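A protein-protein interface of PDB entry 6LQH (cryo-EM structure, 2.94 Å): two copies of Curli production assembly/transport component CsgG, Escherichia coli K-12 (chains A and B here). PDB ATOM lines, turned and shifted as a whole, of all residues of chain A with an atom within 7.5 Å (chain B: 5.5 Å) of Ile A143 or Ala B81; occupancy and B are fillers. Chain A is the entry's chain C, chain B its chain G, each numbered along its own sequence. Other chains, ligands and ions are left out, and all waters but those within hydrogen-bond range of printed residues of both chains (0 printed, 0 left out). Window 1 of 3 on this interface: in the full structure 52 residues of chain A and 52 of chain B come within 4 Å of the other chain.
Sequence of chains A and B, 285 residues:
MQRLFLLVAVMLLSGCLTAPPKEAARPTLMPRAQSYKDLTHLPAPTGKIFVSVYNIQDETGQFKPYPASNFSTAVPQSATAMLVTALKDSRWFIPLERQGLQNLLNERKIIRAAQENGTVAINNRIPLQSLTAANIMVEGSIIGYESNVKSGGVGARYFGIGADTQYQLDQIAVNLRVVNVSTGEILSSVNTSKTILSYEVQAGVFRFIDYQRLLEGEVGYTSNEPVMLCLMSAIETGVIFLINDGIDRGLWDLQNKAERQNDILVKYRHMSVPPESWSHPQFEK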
ATOM      1  N   GLN A  57      16.327 -10.953  16.927  1.00  0.00           N
ATOM      2  CA  GLN A  57      17.069  -9.905  16.256  1.00  0.00           C
ATOM      3  C   GLN A  57      16.969  -8.591  17.014  1.00  0.00           C
ATOM      4  O   GLN A  57      15.974  -8.305  17.677  1.00  0.00           O
ATOM      5  CB  GLN A  57      16.558  -9.725  14.832  1.00  0.00           C
ATOM      6  CG  GLN A  57      17.550  -9.085  13.898  1.00  0.00           C
ATOM      7  CD  GLN A  57      16.899  -8.621  12.617  1.00  0.00           C
ATOM      8  OE1 GLN A  57      15.906  -9.196  12.173  1.00  0.00           O
ATOM      9  NE2 GLN A  57      17.440  -7.565  12.024  1.00  0.00           N
ATOM     10  N   ASP A  58      18.025  -7.791  16.910  1.00  0.00           N
ATOM     11  CA  ASP A  58      18.080  -6.471  17.526  1.00  0.00           C
ATOM     12  C   ASP A  58      17.460  -5.472  16.558  1.00  0.00           C
ATOM     13  O   ASP A  58      18.139  -4.777  15.800  1.00  0.00           O
ATOM     14  CB  ASP A  58      19.514  -6.116  17.873  1.00  0.00           C
ATOM     15  CG  ASP A  58      19.654  -4.722  18.421  1.00  0.00           C
ATOM     16  OD1 ASP A  58      20.081  -3.816  17.673  1.00  0.00           O
ATOM     17  OD2 ASP A  58      19.339  -4.534  19.609  1.00  0.00           O
ATOM     18  N   GLU A  59      16.136  -5.411  16.580  1.00  0.00           N
ATOM     19  CA  GLU A  59      15.396  -4.537  15.686  1.00  0.00           C
ATOM     20  C   GLU A  59      15.228  -3.135  16.240  1.00  0.00           C
ATOM     21  O   GLU A  59      14.302  -2.435  15.831  1.00  0.00           O
ATOM     22  CB  GLU A  59      14.022  -5.131  15.388  1.00  0.00           C
ATOM     23  CG  GLU A  59      14.050  -6.341  14.481  1.00  0.00           C
ATOM     24  CD  GLU A  59      12.666  -6.770  14.038  1.00  0.00           C
ATOM     25  OE1 GLU A  59      12.294  -6.482  12.881  1.00  0.00           O
ATOM     26  OE2 GLU A  59      11.939  -7.380  14.849  1.00  0.00           O
ATOM     27  N   THR A  60      16.088  -2.709  17.160  1.00  0.00           N
ATOM     28  CA  THR A  60      15.937  -1.383  17.736  1.00  0.00           C
ATOM     29  C   THR A  60      16.500  -0.304  16.825  1.00  0.00           C
ATOM     30  O   THR A  60      16.046   0.843  16.873  1.00  0.00           O
ATOM     31  CB  THR A  60      16.610  -1.333  19.102  1.00  0.00           C
ATOM     32  OG1 THR A  60      16.520  -0.008  19.619  1.00  0.00           O
ATOM     33  CG2 THR A  60      18.052  -1.701  18.987  1.00  0.00           C
ATOM     34  N   GLY A  61      17.478  -0.645  15.992  1.00  0.00           N
ATOM     35  CA  GLY A  61      18.081   0.310  15.090  1.00  0.00           C
ATOM     36  C   GLY A  61      18.949   1.358  15.738  1.00  0.00           C
ATOM     37  O   GLY A  61      19.417   2.260  15.043  1.00  0.00           O
ATOM     38  N   GLY A 140      11.186 -13.401  18.272  1.00  0.00           N
ATOM     39  CA  GLY A 140      11.198 -12.192  19.061  1.00  0.00           C
ATOM     40  C   GLY A 140      12.221 -11.212  18.546  1.00  0.00           C
ATOM     41  O   GLY A 140      12.908 -11.449  17.559  1.00  0.00           O
ATOM     42  N   SER A 141      12.289 -10.091  19.244  1.00  0.00           N
ATOM     43  CA  SER A 141      13.232  -9.041  18.916  1.00  0.00           C
ATOM     44  C   SER A 141      13.432  -8.168  20.134  1.00  0.00           C
ATOM     45  O   SER A 141      12.684  -8.244  21.107  1.00  0.00           O
ATOM     46  CB  SER A 141      12.753  -8.183  17.745  1.00  0.00           C
ATOM     47  OG  SER A 141      11.574  -8.697  17.161  1.00  0.00           O
ATOM     48  N   ILE A 142      14.465  -7.339  20.075  1.00  0.00           N
ATOM     49  CA  ILE A 142      14.581  -6.174  20.935  1.00  0.00           C
ATOM     50  C   ILE A 142      13.906  -5.054  20.161  1.00  0.00           C
ATOM     51  O   ILE A 142      14.478  -4.496  19.228  1.00  0.00           O
ATOM     52  CB  ILE A 142      16.032  -5.853  21.279  1.00  0.00           C
ATOM     53  CG1 ILE A 142      16.699  -7.070  21.904  1.00  0.00           C
ATOM     54  CG2 ILE A 142      16.091  -4.699  22.240  1.00  0.00           C
ATOM     55  CD1 ILE A 142      18.118  -7.269  21.473  1.00  0.00           C
ATOM     56  N   ILE A 143      12.666  -4.744  20.532  1.00  0.00           N
ATOM     57  CA  ILE A 143      11.846  -3.869  19.703  1.00  0.00           C
ATOM     58  C   ILE A 143      12.156  -2.398  19.885  1.00  0.00           C
ATOM     59  O   ILE A 143      11.692  -1.579  19.087  1.00  0.00           O
ATOM     60  CB  ILE A 143      10.340  -4.073  19.952  1.00  0.00           C
ATOM     61  CG1 ILE A 143      10.025  -4.046  21.436  1.00  0.00           C
ATOM     62  CG2 ILE A 143       9.874  -5.356  19.325  1.00  0.00           C
ATOM     63  CD1 ILE A 143       8.595  -3.724  21.730  1.00  0.00           C
ATOM     64  N   GLY A 144      12.918  -2.030  20.898  1.00  0.00           N
ATOM     65  CA  GLY A 144      13.207  -0.628  21.072  1.00  0.00           C
ATOM     66  C   GLY A 144      14.170  -0.339  22.193  1.00  0.00           C
ATOM     67  O   GLY A 144      14.136  -0.990  23.236  1.00  0.00           O
ATOM     68  N   TYR A 145      15.043   0.635  21.978  1.00  0.00           N
ATOM     69  CA  TYR A 145      15.926   1.149  23.016  1.00  0.00           C
ATOM     70  C   TYR A 145      15.801   2.666  22.991  1.00  0.00           C
ATOM     71  O   TYR A 145      16.132   3.309  21.993  1.00  0.00           O
ATOM     72  CB  TYR A 145      17.367   0.706  22.806  1.00  0.00           C
ATOM     73  CG  TYR A 145      18.300   1.204  23.876  1.00  0.00           C
ATOM     74  CD1 TYR A 145      18.485   0.493  25.044  1.00  0.00           C
ATOM     75  CD2 TYR A 145      18.982   2.392  23.726  1.00  0.00           C
ATOM     76  CE1 TYR A 145      19.323   0.947  26.020  1.00  0.00           C
ATOM     77  CE2 TYR A 145      19.821   2.853  24.699  1.00  0.00           C
ATOM     78  CZ  TYR A 145      19.988   2.126  25.843  1.00  0.00           C
ATOM     79  OH  TYR A 145      20.832   2.586  26.821  1.00  0.00           O
ATOM     80  N   ILE A 172      14.575  -0.355  27.529  1.00  0.00           N
ATOM     81  CA  ILE A 172      14.740  -1.391  26.524  1.00  0.00           C
ATOM     82  C   ILE A 172      13.489  -2.252  26.533  1.00  0.00           C
ATOM     83  O   ILE A 172      13.022  -2.664  27.597  1.00  0.00           O
ATOM     84  CB  ILE A 172      16.008  -2.225  26.775  1.00  0.00           C
ATOM     85  CG1 ILE A 172      16.141  -3.325  25.733  1.00  0.00           C
ATOM     86  CG2 ILE A 172      16.020  -2.797  28.176  1.00  0.00           C
ATOM     87  CD1 ILE A 172      17.525  -3.842  25.609  1.00  0.00           C
ATOM     88  N   ALA A 173      12.930  -2.497  25.357  1.00  0.00           N
ATOM     89  CA  ALA A 173      11.722  -3.292  25.223  1.00  0.00           C
ATOM     90  C   ALA A 173      12.028  -4.505  24.367  1.00  0.00           C
ATOM     91  O   ALA A 173      12.721  -4.393  23.357  1.00  0.00           O
ATOM     92  CB  ALA A 173      10.590  -2.476  24.609  1.00  0.00           C
ATOM     93  N   VAL A 174      11.518  -5.659  24.776  1.00  0.00           N
ATOM     94  CA  VAL A 174      11.744  -6.925  24.098  1.00  0.00           C
ATOM     95  C   VAL A 174      10.392  -7.543  23.787  1.00  0.00           C
ATOM     96  O   VAL A 174       9.537  -7.644  24.667  1.00  0.00           O
ATOM     97  CB  VAL A 174      12.589  -7.881  24.956  1.00  0.00           C
ATOM     98  CG1 VAL A 174      13.036  -9.063  24.140  1.00  0.00           C
ATOM     99  CG2 VAL A 174      13.784  -7.162  25.513  1.00  0.00           C
ATOM    100  N   ASN A 175      10.203  -7.956  22.545  1.00  0.00           N
ATOM    101  CA  ASN A 175       9.010  -8.681  22.143  1.00  0.00           C
ATOM    102  C   ASN A 175       9.348 -10.152  21.995  1.00  0.00           C
ATOM    103  O   ASN A 175      10.335 -10.507  21.350  1.00  0.00           O
ATOM    104  CB  ASN A 175       8.466  -8.138  20.827  1.00  0.00           C
ATOM    105  CG  ASN A 175       7.472  -9.059  20.186  1.00  0.00           C
ATOM    106  OD1 ASN A 175       7.792  -9.770  19.242  1.00  0.00           O
ATOM    107  ND2 ASN A 175       6.249  -9.040  20.681  1.00  0.00           N
ATOM    108  N   LEU A 176       8.531 -11.004  22.607  1.00  0.00           N
ATOM    109  CA  LEU A 176       8.707 -12.447  22.526  1.00  0.00           C
ATOM    110  C   LEU A 176       7.414 -13.070  22.038  1.00  0.00           C
ATOM    111  O   LEU A 176       6.352 -12.800  22.599  1.00  0.00           O
ATOM    112  CB  LEU A 176       9.089 -13.040  23.881  1.00  0.00           C
ATOM    113  CG  LEU A 176      10.531 -12.900  24.347  1.00  0.00           C
ATOM    114  CD1 LEU A 176      10.659 -11.720  25.268  1.00  0.00           C
ATOM    115  CD2 LEU A 176      10.928 -14.147  25.062  1.00  0.00           C
ATOM    116  N   ARG A 177       7.503 -13.906  21.010  1.00  0.00           N
ATOM    117  CA  ARG A 177       6.350 -14.573  20.425  1.00  0.00           C
ATOM    118  C   ARG A 177       6.548 -16.076  20.504  1.00  0.00           C
ATOM    119  O   ARG A 177       7.540 -16.601  19.998  1.00  0.00           O
ATOM    120  CB  ARG A 177       6.151 -14.161  18.971  1.00  0.00           C
ATOM    121  CG  ARG A 177       6.169 -12.687  18.746  1.00  0.00           C
ATOM    122  CD  ARG A 177       6.121 -12.366  17.277  1.00  0.00           C
ATOM    123  NE  ARG A 177       7.324 -11.671  16.850  1.00  0.00           N
ATOM    124  CZ  ARG A 177       8.076 -12.056  15.829  1.00  0.00           C
ATOM    125  NH1 ARG A 177       7.739 -13.129  15.132  1.00  0.00           N
ATOM    126  NH2 ARG A 177       9.158 -11.368  15.503  1.00  0.00           N
ATOM    127  N   SER A 189       2.226 -13.425  22.344  1.00  0.00           N
ATOM    128  CA  SER A 189       3.185 -12.371  22.035  1.00  0.00           C
ATOM    129  C   SER A 189       3.150 -11.364  23.172  1.00  0.00           C
ATOM    130  O   SER A 189       2.089 -10.820  23.483  1.00  0.00           O
ATOM    131  CB  SER A 189       2.865 -11.706  20.705  1.00  0.00           C
ATOM    132  OG  SER A 189       3.639 -10.537  20.532  1.00  0.00           O
ATOM    133  N   VAL A 190       4.300 -11.128  23.792  1.00  0.00           N
ATOM    134  CA  VAL A 190       4.414 -10.225  24.927  1.00  0.00           C
ATOM    135  C   VAL A 190       5.470  -9.178  24.612  1.00  0.00           C
ATOM    136  O   VAL A 190       6.427  -9.449  23.880  1.00  0.00           O
ATOM    137  CB  VAL A 190       4.756 -10.989  26.222  1.00  0.00           C
ATOM    138  CG1 VAL A 190       6.151 -11.558  26.151  1.00  0.00           C
ATOM    139  CG2 VAL A 190       4.610 -10.088  27.427  1.00  0.00           C
ATOM    140  N   ASN A 191       5.277  -7.974  25.140  1.00  0.00           N
ATOM    141  CA  ASN A 191       6.253  -6.895  25.059  1.00  0.00           C
ATOM    142  C   ASN A 191       6.639  -6.514  26.482  1.00  0.00           C
ATOM    143  O   ASN A 191       5.812  -5.999  27.238  1.00  0.00           O
ATOM    144  CB  ASN A 191       5.688  -5.698  24.303  1.00  0.00           C
ATOM    145  CG  ASN A 191       5.610  -5.935  22.816  1.00  0.00           C
ATOM    146  OD1 ASN A 191       5.850  -7.039  22.341  1.00  0.00           O
ATOM    147  ND2 ASN A 191       5.265  -4.898  22.070  1.00  0.00           N
ATOM    148  N   THR A 192       7.888  -6.773  26.844  1.00  0.00           N
ATOM    149  CA  THR A 192       8.406  -6.491  28.174  1.00  0.00           C
ATOM    150  C   THR A 192       9.358  -5.309  28.114  1.00  0.00           C
ATOM    151  O   THR A 192      10.272  -5.288  27.292  1.00  0.00           O
ATOM    152  CB  THR A 192       9.138  -7.703  28.739  1.00  0.00           C
ATOM    153  OG1 THR A 192       8.318  -8.865  28.597  1.00  0.00           O
ATOM    154  CG2 THR A 192       9.462  -7.485  30.197  1.00  0.00           C
ATOM    155  N   SER A 193       9.160  -4.340  28.994  1.00  0.00           N
ATOM    156  CA  SER A 193      10.034  -3.184  29.065  1.00  0.00           C
ATOM    157  C   SER A 193      10.847  -3.237  30.349  1.00  0.00           C
ATOM    158  O   SER A 193      10.408  -3.790  31.360  1.00  0.00           O
ATOM    159  CB  SER A 193       9.242  -1.880  28.997  1.00  0.00           C
ATOM    160  OG  SER A 193       9.730  -0.937  29.932  1.00  0.00           O
ATOM    161  N   LEU A 231      18.684  -6.278  29.513  1.00  0.00           N
ATOM    162  CA  LEU A 231      18.119  -7.082  28.440  1.00  0.00           C
ATOM    163  C   LEU A 231      17.861  -8.509  28.897  1.00  0.00           C
ATOM    164  O   LEU A 231      16.833  -9.093  28.544  1.00  0.00           O
ATOM    165  CB  LEU A 231      19.056  -7.060  27.238  1.00  0.00           C
ATOM    166  CG  LEU A 231      18.717  -7.964  26.061  1.00  0.00           C
ATOM    167  CD1 LEU A 231      17.352  -7.624  25.527  1.00  0.00           C
ATOM    168  CD2 LEU A 231      19.759  -7.825  24.981  1.00  0.00           C
ATOM    169  N   PRO B  76      12.230   2.966  15.778  1.00  0.00           N
ATOM    170  CA  PRO B  76      12.611   1.554  15.828  1.00  0.00           C
ATOM    171  C   PRO B  76      12.309   0.848  14.518  1.00  0.00           C
ATOM    172  O   PRO B  76      11.290   1.089  13.874  1.00  0.00           O
ATOM    173  CB  PRO B  76      11.753   1.000  16.964  1.00  0.00           C
ATOM    174  CG  PRO B  76      11.454   2.161  17.808  1.00  0.00           C
ATOM    175  CD  PRO B  76      11.382   3.349  16.917  1.00  0.00           C
ATOM    176  N   GLN B  77      13.210  -0.050  14.133  1.00  0.00           N
ATOM    177  CA  GLN B  77      12.987  -0.921  12.992  1.00  0.00           C
ATOM    178  C   GLN B  77      12.124  -2.114  13.347  1.00  0.00           C
ATOM    179  O   GLN B  77      12.181  -3.142  12.668  1.00  0.00           O
ATOM    180  CB  GLN B  77      14.316  -1.397  12.407  1.00  0.00           C
ATOM    181  CG  GLN B  77      15.396  -0.348  12.234  1.00  0.00           C
ATOM    182  CD  GLN B  77      14.993   0.815  11.345  1.00  0.00           C
ATOM    183  OE1 GLN B  77      13.937   1.413  11.505  1.00  0.00           O
ATOM    184  NE2 GLN B  77      15.823   1.101  10.360  1.00  0.00           N
ATOM    185  N   SER B  78      11.324  -1.993  14.399  1.00  0.00           N
ATOM    186  CA  SER B  78      10.662  -3.123  15.024  1.00  0.00           C
ATOM    187  C   SER B  78       9.148  -3.017  15.015  1.00  0.00           C
ATOM    188  O   SER B  78       8.494  -3.595  15.883  1.00  0.00           O
ATOM    189  CB  SER B  78      11.153  -3.265  16.452  1.00  0.00           C
ATOM    190  OG  SER B  78      10.417  -2.391  17.277  1.00  0.00           O
ATOM    191  N   ALA B  79       8.574  -2.279  14.076  1.00  0.00           N
ATOM    192  CA  ALA B  79       7.212  -2.596  13.702  1.00  0.00           C
ATOM    193  C   ALA B  79       7.217  -3.955  13.012  1.00  0.00           C
ATOM    194  O   ALA B  79       8.272  -4.489  12.662  1.00  0.00           O
ATOM    195  CB  ALA B  79       6.634  -1.515  12.801  1.00  0.00           C
ATOM    196  N   THR B  80       6.026  -4.511  12.806  1.00  0.00           N
ATOM    197  CA  THR B  80       5.744  -5.909  12.502  1.00  0.00           C
ATOM    198  C   THR B  80       5.858  -6.753  13.755  1.00  0.00           C
ATOM    199  O   THR B  80       5.463  -7.912  13.737  1.00  0.00           O
ATOM    200  CB  THR B  80       6.662  -6.517  11.422  1.00  0.00           C
ATOM    201  OG1 THR B  80       7.024  -5.514  10.472  1.00  0.00           O
ATOM    202  CG2 THR B  80       5.974  -7.648  10.702  1.00  0.00           C
ATOM    203  N   ALA B  81       6.367  -6.209  14.849  1.00  0.00           N
ATOM    204  CA  ALA B  81       6.305  -6.830  16.159  1.00  0.00           C
ATOM    205  C   ALA B  81       5.438  -6.037  17.109  1.00  0.00           C
ATOM    206  O   ALA B  81       4.728  -6.618  17.925  1.00  0.00           O
ATOM    207  CB  ALA B  81       7.710  -6.973  16.745  1.00  0.00           C
ATOM    208  N   MET B  82       5.484  -4.711  17.003  1.00  0.00           N
ATOM    209  CA  MET B  82       4.481  -3.880  17.646  1.00  0.00           C
ATOM    210  C   MET B  82       3.128  -4.045  16.981  1.00  0.00           C
ATOM    211  O   MET B  82       2.098  -3.987  17.655  1.00  0.00           O
ATOM    212  CB  MET B  82       4.910  -2.417  17.606  1.00  0.00           C
ATOM    213  CG  MET B  82       6.269  -2.155  18.199  1.00  0.00           C
ATOM    214  SD  MET B  82       6.638  -0.403  18.240  1.00  0.00           S
ATOM    215  CE  MET B  82       8.315  -0.437  18.841  1.00  0.00           C
ATOM    216  N   LEU B  83       3.107  -4.268  15.668  1.00  0.00           N
ATOM    217  CA  LEU B  83       1.840  -4.448  14.974  1.00  0.00           C
ATOM    218  C   LEU B  83       1.262  -5.831  15.214  1.00  0.00           C
ATOM    219  O   LEU B  83       0.058  -5.970  15.424  1.00  0.00           O
ATOM    220  CB  LEU B  83       2.008  -4.213  13.478  1.00  0.00           C
ATOM    221  CG  LEU B  83       0.728  -4.500  12.701  1.00  0.00           C
ATOM    222  CD1 LEU B  83      -0.381  -3.638  13.215  1.00  0.00           C
ATOM    223  CD2 LEU B  83       0.917  -4.248  11.252  1.00  0.00           C
ATOM    224  N   VAL B  84       2.095  -6.869  15.157  1.00  0.00           N
ATOM    225  CA  VAL B  84       1.617  -8.208  15.472  1.00  0.00           C
ATOM    226  C   VAL B  84       1.101  -8.261  16.899  1.00  0.00           C
ATOM    227  O   VAL B  84       0.076  -8.891  17.174  1.00  0.00           O
ATOM    228  CB  VAL B  84       2.734  -9.234  15.222  1.00  0.00           C
ATOM    229  CG1 VAL B  84       2.559 -10.441  16.105  1.00  0.00           C
ATOM    230  CG2 VAL B  84       2.749  -9.638  13.773  1.00  0.00           C
ATOM    231  N   THR B  85       1.770  -7.575  17.821  1.00  0.00           N
ATOM    232  CA  THR B  85       1.283  -7.511  19.192  1.00  0.00           C
ATOM    233  C   THR B  85       0.001  -6.701  19.301  1.00  0.00           C
ATOM    234  O   THR B  85      -0.875  -7.045  20.095  1.00  0.00           O
ATOM    235  CB  THR B  85       2.352  -6.922  20.103  1.00  0.00           C
ATOM    236  OG1 THR B  85       3.609  -7.538  19.815  1.00  0.00           O
ATOM    237  CG2 THR B  85       2.009  -7.166  21.547  1.00  0.00           C
ATOM    238  N   ALA B  86      -0.132  -5.627  18.524  1.00  0.00           N
ATOM    239  CA  ALA B  86      -1.365  -4.849  18.556  1.00  0.00           C
ATOM    240  C   ALA B  86      -2.539  -5.639  18.005  1.00  0.00           C
ATOM    241  O   ALA B  86      -3.660  -5.512  18.504  1.00  0.00           O
ATOM    242  CB  ALA B  86      -1.191  -3.554  17.773  1.00  0.00           C
ATOM    243  N   GLN B  99       6.970 -13.423   9.386  1.00  0.00           N
ATOM    244  CA  GLN B  99       8.153 -12.593   9.602  1.00  0.00           C
ATOM    245  C   GLN B  99       9.030 -13.434  10.511  1.00  0.00           C
ATOM    246  O   GLN B  99       8.945 -13.340  11.736  1.00  0.00           O
ATOM    247  CB  GLN B  99       7.811 -11.253  10.218  1.00  0.00           C
ATOM    248  CG  GLN B  99       9.020 -10.384  10.478  1.00  0.00           C
ATOM    249  CD  GLN B  99       9.035  -9.819  11.877  1.00  0.00           C
ATOM    250  OE1 GLN B  99       8.123 -10.061  12.666  1.00  0.00           O
ATOM    251  NE2 GLN B  99      10.077  -9.063  12.197  1.00  0.00           N
ATOM    252  N   MET B 228       9.441   4.341  20.792  1.00  0.00           N
ATOM    253  CA  MET B 228       8.811   3.034  20.681  1.00  0.00           C
ATOM    254  C   MET B 228       7.425   3.018  21.304  1.00  0.00           C
ATOM    255  O   MET B 228       6.518   2.407  20.740  1.00  0.00           O
ATOM    256  CB  MET B 228       9.685   1.957  21.317  1.00  0.00           C
ATOM    257  CG  MET B 228      10.298   2.364  22.634  1.00  0.00           C
ATOM    258  SD  MET B 228      11.114   1.015  23.493  1.00  0.00           S
ATOM    259  CE  MET B 228      11.746   1.885  24.914  1.00  0.00           C
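The guanidinium group (NH2) of Arg A177 lies within hydrogen-bond range of the side-chain amide oxygen (OE1) of Gln B99 (3.3 Å). NE2 of Gln B99 lies within hydrogen-bond range of OE1 of Glu A59 (3.5 Å). OD1 of Asn A191 lies within hydrogen-bond range of OG1 of Thr B85. N of Gln B77 is in hydrogen-bond range of O of Glu A59, 3.1 Å away. The side-chain amide nitrogen (ND2) of Asn A175 sits at hydrogen-bond distance from the side-chain hydroxyl (OG1) of Thr B85 (3.2 Å). The side-chain hydroxyl of Thr B85 is in hydrogen-bond range of the side-chain hydroxyl of Ser A189, at 3.1 Å. The side-chain hydroxyl (OG) of Ser B78 lies close to the backbone carbonyl oxygen (O) of Ile A143, 2.4 Å away. N of Ser B78 sits close to O of Glu A59. The backbone carbonyl oxygen (O) of Gly A144 sits close to the side-chain sulfur (SD) of Met B228.
The guanidinium group (NE) of Arg A177 sits at hydrogen-bond distance from the side-chain amide oxygen (OD1) of Asn A175, 3.1 Å away. ND2 of Asn A175 sits close to O of Val A190, at 3.2 Å. ND2 of Asn A175 sits at hydrogen-bond distance from OG of Ser A189, 3.0 Å away. N of Glu A59 is in hydrogen-bond range of O of Ile A142, at 3.3 Å. O of Ser A141 sits at hydrogen-bond distance from N of Asn A175 (2.9 Å). OE2 of Glu A59 sits at hydrogen-bond distance from OG of Ser A141 (2.7 Å).
Among the printed residues, pairs that only touch across the chains: Ile A143 with Pro B76 (3.3 Å), Ile A143 with Met B82 (3.6 Å), Thr A60 with Pro B76 (3.7 Å), Ala A173 with Met B228 (3.7 Å), Ile A143 with Ala B81 (3.7 Å), Asn A175 with Ala B81 (3.8 Å) and Gly A61 with Gln B77 (3.97 Å).
Of the printed residues of chain B, Glu A59 touches Gln B77 (3.1 Å), Ser B78 (3.3 Å) and Gln B99 (3.5 Å). Of the printed residues of chain B, Asn A175 touches Ala B81 (3.8 Å) and Thr B85 (3.2 Å). Printed residues of chain B within 4 Å of Ser A189: Thr B85. Ser A193 touches none of the printed residues of chain B. Printed residues of chain A within 4 Å of Pro B76: Thr A60 and Ile A143. Of chain A, only Ile A143 and Asn A175 come within 4 Å of Ala B81. Printed residues of chain A within 4 Å of Thr B85: Asn A175, Ser A189 and Asn A191. The nearest printed residue of chain B that does not touch Gly A144 is Ser B78 (4.4 Å).
Of the 23 printed residues of chain A, 10 touch a printed residue of chain B. Hydrophobic or aromatic side chains of chain A within 4 Å of the printed part of chain B: Ile A143 and Ala A173. Among the printed residues, no Asp or Glu carboxylate lies within 4 Å of a Lys or Arg side-chain nitrogen of the other chain.
No position is printed for both chains.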
